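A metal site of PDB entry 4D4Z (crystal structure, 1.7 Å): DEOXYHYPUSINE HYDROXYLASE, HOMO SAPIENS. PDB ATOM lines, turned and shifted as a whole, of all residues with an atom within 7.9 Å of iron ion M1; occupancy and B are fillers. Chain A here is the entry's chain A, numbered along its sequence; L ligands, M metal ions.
The side-chain carboxylate (OE1) of Glu 95 is bound to iron ion M1. An oxygen (O1) of LG2 L2 is bound to iron ion M1, 2.1 Å away. Iron ion M1 is bound by O3 of LIG L1, at 2.1 Å. Iron ion M1 is bound by a ring nitrogen (NE2) of His 212 (2.2 Å). O2 of LIG L1 is bound to iron ion M1 (2.2 Å). NE2 of His 94 binds iron ion M1, at 2.2 Å. Iron ion M1 has six donor atoms within binding distance.
Three residues have an atom within 4 Å of iron ion M1: His 94, Glu 95 and His 212. The nearest printed residue that does not touch iron ion M1 is Glu 246 (4.1 Å).
A ring nitrogen (ND1) of His 212 lies within hydrogen-bond range of the backbone carbonyl oxygen (O) of Leu 209, 2.8 Å away. A ring nitrogen (ND1) of His 94 sits at hydrogen-bond distance from the side-chain hydroxyl (OG1) of Thr 126, at 2.8 Å.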
ATOM      1  N   HIS A  61       9.764 -29.963 -21.809  1.00  0.00           N
ATOM      2  CA  HIS A  61       8.434 -30.278 -21.303  1.00  0.00           C
ATOM      3  C   HIS A  61       7.418 -30.364 -22.470  1.00  0.00           C
ATOM      4  O   HIS A  61       6.532 -31.170 -22.449  1.00  0.00           O
ATOM      5  CB  HIS A  61       8.040 -29.376 -20.126  1.00  0.00           C
ATOM      6  CG  HIS A  61       7.004 -28.349 -20.399  1.00  0.00           C
ATOM      7  ND1 HIS A  61       7.160 -27.343 -21.314  1.00  0.00           N
ATOM      8  CD2 HIS A  61       5.782 -28.159 -19.864  1.00  0.00           C
ATOM      9  CE1 HIS A  61       6.104 -26.565 -21.312  1.00  0.00           C
ATOM     10  NE2 HIS A  61       5.243 -27.043 -20.446  1.00  0.00           N
ATOM     11  N   GLU A  62       7.624 -29.552 -23.513  1.00  0.00           N
ATOM     12  CA  GLU A  62       6.738 -29.611 -24.685  1.00  0.00           C
ATOM     13  C   GLU A  62       6.945 -30.956 -25.433  1.00  0.00           C
ATOM     14  O   GLU A  62       5.944 -31.470 -26.007  1.00  0.00           O
ATOM     15  CB  GLU A  62       6.942 -28.512 -25.663  1.00  0.00           C
ATOM     16  CG  GLU A  62       5.696 -28.152 -26.409  1.00  0.00           C
ATOM     17  CD  GLU A  62       4.732 -27.326 -25.537  1.00  0.00           C
ATOM     18  OE1 GLU A  62       4.841 -27.341 -24.297  1.00  0.00           O
ATOM     19  OE2 GLU A  62       3.879 -26.613 -26.063  1.00  0.00           O
ATOM     20  N   TYR A  65       4.690 -33.249 -23.555  1.00  0.00           N
ATOM     21  CA  TYR A  65       3.300 -32.893 -23.821  1.00  0.00           C
ATOM     22  C   TYR A  65       2.887 -33.486 -25.149  1.00  0.00           C
ATOM     23  O   TYR A  65       1.845 -34.166 -25.223  1.00  0.00           O
ATOM     24  CB  TYR A  65       3.081 -31.368 -23.833  1.00  0.00           C
ATOM     25  CG  TYR A  65       1.666 -30.966 -24.216  1.00  0.00           C
ATOM     26  CD1 TYR A  65       0.618 -31.032 -23.278  1.00  0.00           C
ATOM     27  CD2 TYR A  65       1.393 -30.524 -25.493  1.00  0.00           C
ATOM     28  CE1 TYR A  65      -0.648 -30.617 -23.628  1.00  0.00           C
ATOM     29  CE2 TYR A  65       0.126 -30.114 -25.813  1.00  0.00           C
ATOM     30  CZ  TYR A  65      -0.846 -30.151 -24.894  1.00  0.00           C
ATOM     31  OH  TYR A  65      -2.148 -29.764 -25.294  1.00  0.00           O
ATOM     32  N   PRO A  90      11.352 -30.127 -12.330  1.00  0.00           N
ATOM     33  CA  PRO A  90       9.991 -30.567 -11.968  1.00  0.00           C
ATOM     34  C   PRO A  90       8.967 -30.473 -13.094  1.00  0.00           C
ATOM     35  O   PRO A  90       8.128 -31.376 -13.253  1.00  0.00           O
ATOM     36  CB  PRO A  90       9.630 -29.708 -10.755  1.00  0.00           C
ATOM     37  CG  PRO A  90      10.968 -29.455 -10.104  1.00  0.00           C
ATOM     38  CD  PRO A  90      11.931 -29.273 -11.284  1.00  0.00           C
ATOM     39  N   MET A  91       8.997 -29.388 -13.834  1.00  0.00           N
ATOM     40  CA  MET A  91       7.956 -29.224 -14.855  1.00  0.00           C
ATOM     41  C   MET A  91       8.128 -30.251 -15.977  1.00  0.00           C
ATOM     42  O   MET A  91       7.117 -30.589 -16.608  1.00  0.00           O
ATOM     43  CB  MET A  91       7.836 -27.834 -15.505  1.00  0.00           C
ATOM     44  CG  MET A  91       9.042 -27.398 -16.341  1.00  0.00           C
ATOM     45  SD  MET A  91       8.869 -25.688 -16.900  1.00  0.00           S
ATOM     46  CE  MET A  91       7.772 -25.624 -18.339  1.00  0.00           C
ATOM     47  N   VAL A  92       9.334 -30.711 -16.242  1.00  0.00           N
ATOM     48  CA  VAL A  92       9.588 -31.691 -17.319  1.00  0.00           C
ATOM     49  C   VAL A  92       9.133 -33.093 -16.807  1.00  0.00           C
ATOM     50  O   VAL A  92       8.442 -33.838 -17.520  1.00  0.00           O
ATOM     51  CB  VAL A  92      11.042 -31.770 -17.731  1.00  0.00           C
ATOM     52  CG1 VAL A  92      11.276 -32.880 -18.704  1.00  0.00           C
ATOM     53  CG2 VAL A  92      11.513 -30.422 -18.290  1.00  0.00           C
ATOM     54  N   HIS A  94       6.844 -33.608 -14.436  1.00  0.00           N
ATOM     55  CA  HIS A  94       5.403 -33.511 -14.397  1.00  0.00           C
ATOM     56  C   HIS A  94       4.818 -33.778 -15.798  1.00  0.00           C
ATOM     57  O   HIS A  94       3.865 -34.523 -15.937  1.00  0.00           O
ATOM     58  CB  HIS A  94       4.933 -32.101 -13.850  1.00  0.00           C
ATOM     59  CG  HIS A  94       3.838 -31.470 -14.659  1.00  0.00           C
ATOM     60  ND1 HIS A  94       2.541 -31.948 -14.724  1.00  0.00           N
ATOM     61  CD2 HIS A  94       3.892 -30.435 -15.527  1.00  0.00           C
ATOM     62  CE1 HIS A  94       1.847 -31.203 -15.573  1.00  0.00           C
ATOM     63  NE2 HIS A  94       2.642 -30.300 -16.087  1.00  0.00           N
ATOM     64  N   GLU A  95       5.396 -33.174 -16.814  1.00  0.00           N
ATOM     65  CA  GLU A  95       4.762 -33.255 -18.117  1.00  0.00           C
ATOM     66  C   GLU A  95       4.836 -34.724 -18.644  1.00  0.00           C
ATOM     67  O   GLU A  95       3.947 -35.246 -19.247  1.00  0.00           O
ATOM     68  CB  GLU A  95       5.382 -32.255 -19.095  1.00  0.00           C
ATOM     69  CG  GLU A  95       4.383 -31.833 -20.153  1.00  0.00           C
ATOM     70  CD  GLU A  95       3.191 -31.027 -19.607  1.00  0.00           C
ATOM     71  OE1 GLU A  95       3.406 -30.055 -18.815  1.00  0.00           O
ATOM     72  OE2 GLU A  95       2.020 -31.473 -19.859  1.00  0.00           O
ATOM     73  N   ALA A  96       5.897 -35.407 -18.246  1.00  0.00           N
ATOM     74  CA  ALA A  96       6.103 -36.836 -18.651  1.00  0.00           C
ATOM     75  C   ALA A  96       5.102 -37.687 -17.908  1.00  0.00           C
ATOM     76  O   ALA A  96       4.512 -38.548 -18.511  1.00  0.00           O
ATOM     77  CB  ALA A  96       7.549 -37.265 -18.343  1.00  0.00           C
ATOM     78  N   GLU A  98       2.168 -36.745 -16.721  1.00  0.00           N
ATOM     79  CA  GLU A  98       0.872 -36.423 -17.286  1.00  0.00           C
ATOM     80  C   GLU A  98       0.706 -37.183 -18.643  1.00  0.00           C
ATOM     81  O   GLU A  98      -0.414 -37.690 -18.920  1.00  0.00           O
ATOM     82  CB  GLU A  98       0.689 -34.895 -17.480  1.00  0.00           C
ATOM     83  CG  GLU A  98      -0.706 -34.567 -18.043  1.00  0.00           C
ATOM     84  CD  GLU A  98      -1.121 -33.110 -18.128  1.00  0.00           C
ATOM     85  OE1 GLU A  98      -0.835 -32.281 -17.254  1.00  0.00           O
ATOM     86  OE2 GLU A  98      -1.892 -32.833 -19.080  1.00  0.00           O
ATOM     87  N   THR A 126       0.744 -34.771 -10.122  1.00  0.00           N
ATOM     88  CA  THR A 126       0.532 -35.175 -11.523  1.00  0.00           C
ATOM     89  C   THR A 126       0.183 -36.660 -11.599  1.00  0.00           C
ATOM     90  O   THR A 126      -0.708 -37.087 -12.313  1.00  0.00           O
ATOM     91  CB  THR A 126       1.809 -34.940 -12.307  1.00  0.00           C
ATOM     92  OG1 THR A 126       1.949 -33.540 -12.521  1.00  0.00           O
ATOM     93  CG2 THR A 126       1.777 -35.585 -13.598  1.00  0.00           C
ATOM     94  N   LEU A 209       0.616 -26.912  -9.236  1.00  0.00           N
ATOM     95  CA  LEU A 209       0.137 -27.671 -10.384  1.00  0.00           C
ATOM     96  C   LEU A 209      -1.254 -27.261 -10.863  1.00  0.00           C
ATOM     97  O   LEU A 209      -1.498 -27.001 -12.073  1.00  0.00           O
ATOM     98  CB  LEU A 209       0.148 -29.189 -10.070  1.00  0.00           C
ATOM     99  CG  LEU A 209      -0.050 -30.035 -11.323  1.00  0.00           C
ATOM    100  CD1 LEU A 209       1.165 -30.097 -12.193  1.00  0.00           C
ATOM    101  CD2 LEU A 209      -0.484 -31.421 -10.920  1.00  0.00           C
ATOM    102  N   HIS A 212      -1.151 -23.821 -12.605  1.00  0.00           N
ATOM    103  CA  HIS A 212      -0.661 -23.930 -13.993  1.00  0.00           C
ATOM    104  C   HIS A 212      -1.700 -24.506 -14.902  1.00  0.00           C
ATOM    105  O   HIS A 212      -1.770 -24.108 -16.087  1.00  0.00           O
ATOM    106  CB  HIS A 212       0.710 -24.673 -13.989  1.00  0.00           C
ATOM    107  CG  HIS A 212       0.780 -25.961 -14.767  1.00  0.00           C
ATOM    108  ND1 HIS A 212       0.178 -27.138 -14.372  1.00  0.00           N
ATOM    109  CD2 HIS A 212       1.459 -26.264 -15.922  1.00  0.00           C
ATOM    110  CE1 HIS A 212       0.440 -28.082 -15.269  1.00  0.00           C
ATOM    111  NE2 HIS A 212       1.245 -27.588 -16.192  1.00  0.00           N
ATOM    112  N   GLU A 213      -2.490 -25.469 -14.437  1.00  0.00           N
ATOM    113  CA  GLU A 213      -3.574 -26.038 -15.272  1.00  0.00           C
ATOM    114  C   GLU A 213      -4.636 -24.976 -15.602  1.00  0.00           C
ATOM    115  O   GLU A 213      -5.144 -24.909 -16.730  1.00  0.00           O
ATOM    116  CB  GLU A 213      -4.169 -27.284 -14.655  1.00  0.00           C
ATOM    117  CG  GLU A 213      -4.906 -28.097 -15.681  1.00  0.00           C
ATOM    118  CD  GLU A 213      -4.029 -28.858 -16.635  1.00  0.00           C
ATOM    119  OE1 GLU A 213      -2.916 -29.171 -16.297  1.00  0.00           O
ATOM    120  OE2 GLU A 213      -4.400 -29.093 -17.825  1.00  0.00           O
ATOM    121  N   TYR A 216      -3.218 -22.954 -18.377  1.00  0.00           N
ATOM    122  CA  TYR A 216      -3.331 -23.713 -19.644  1.00  0.00           C
ATOM    123  C   TYR A 216      -4.757 -23.624 -20.211  1.00  0.00           C
ATOM    124  O   TYR A 216      -4.929 -23.305 -21.406  1.00  0.00           O
ATOM    125  CB  TYR A 216      -2.978 -25.142 -19.365  1.00  0.00           C
ATOM    126  CG  TYR A 216      -3.285 -26.088 -20.494  1.00  0.00           C
ATOM    127  CD1 TYR A 216      -2.437 -26.199 -21.547  1.00  0.00           C
ATOM    128  CD2 TYR A 216      -4.319 -26.995 -20.408  1.00  0.00           C
ATOM    129  CE1 TYR A 216      -2.656 -27.133 -22.593  1.00  0.00           C
ATOM    130  CE2 TYR A 216      -4.562 -27.914 -21.459  1.00  0.00           C
ATOM    131  CZ  TYR A 216      -3.713 -27.961 -22.526  1.00  0.00           C
ATOM    132  OH  TYR A 216      -3.953 -28.968 -23.495  1.00  0.00           O
ATOM    133  N   MET A 242       6.658 -22.721 -13.335  1.00  0.00           N
ATOM    134  CA  MET A 242       5.712 -23.455 -14.157  1.00  0.00           C
ATOM    135  C   MET A 242       4.391 -22.689 -14.342  1.00  0.00           C
ATOM    136  O   MET A 242       3.786 -22.712 -15.415  1.00  0.00           O
ATOM    137  CB  MET A 242       5.405 -24.835 -13.584  1.00  0.00           C
ATOM    138  CG  MET A 242       4.585 -25.716 -14.496  1.00  0.00           C
ATOM    139  SD  MET A 242       4.238 -27.295 -13.683  1.00  0.00           S
ATOM    140  CE  MET A 242       5.780 -27.594 -12.883  1.00  0.00           C
ATOM    141  N   HIS A 245       5.074 -19.516 -16.589  1.00  0.00           N
ATOM    142  CA  HIS A 245       5.212 -19.929 -18.007  1.00  0.00           C
ATOM    143  C   HIS A 245       3.880 -20.168 -18.635  1.00  0.00           C
ATOM    144  O   HIS A 245       3.572 -19.701 -19.731  1.00  0.00           O
ATOM    145  CB  HIS A 245       6.169 -21.136 -18.047  1.00  0.00           C
ATOM    146  CG  HIS A 245       5.592 -22.300 -18.743  1.00  0.00           C
ATOM    147  ND1 HIS A 245       5.529 -22.324 -20.131  1.00  0.00           N
ATOM    148  CD2 HIS A 245       5.052 -23.451 -18.311  1.00  0.00           C
ATOM    149  CE1 HIS A 245       4.931 -23.444 -20.517  1.00  0.00           C
ATOM    150  NE2 HIS A 245       4.655 -24.142 -19.426  1.00  0.00           N
ATOM    151  N   GLU A 246       2.948 -20.857 -17.960  1.00  0.00           N
ATOM    152  CA  GLU A 246       1.709 -21.198 -18.527  1.00  0.00           C
ATOM    153  C   GLU A 246       0.865 -19.939 -18.719  1.00  0.00           C
ATOM    154  O   GLU A 246       0.134 -19.759 -19.729  1.00  0.00           O
ATOM    155  CB  GLU A 246       1.043 -22.286 -17.662  1.00  0.00           C
ATOM    156  CG  GLU A 246       0.255 -23.260 -18.394  1.00  0.00           C
ATOM    157  CD  GLU A 246       1.070 -24.184 -19.272  1.00  0.00           C
ATOM    158  OE1 GLU A 246       2.007 -24.891 -18.804  1.00  0.00           O
ATOM    159  OE2 GLU A 246       0.728 -24.145 -20.472  1.00  0.00           O
HETATM  160  C1  LIG L   1      -1.402 -29.525 -19.872  1.00  0.00           C
HETATM  161  O1  LIG L   1      -2.499 -30.266 -19.185  1.00  0.00           O
HETATM  162  C2  LIG L   1      -0.381 -28.898 -18.957  1.00  0.00           C
HETATM  163  O2  LIG L   1       0.536 -29.865 -18.302  1.00  0.00           O
HETATM  164  C3  LIG L   1       0.448 -27.845 -19.719  1.00  0.00           C
HETATM  165  O3  LIG L   1       1.813 -27.765 -19.417  1.00  0.00           O
HETATM  166  O1  LG2 L   2       3.775 -27.339 -17.681  1.00  0.00           O
HETATM  167 FE    FE M   1       2.317 -28.782 -17.659  1.00  0.00          FE
HETATM  168 FE    FE M   2       3.452 -26.087 -19.478  1.00  0.00          FE
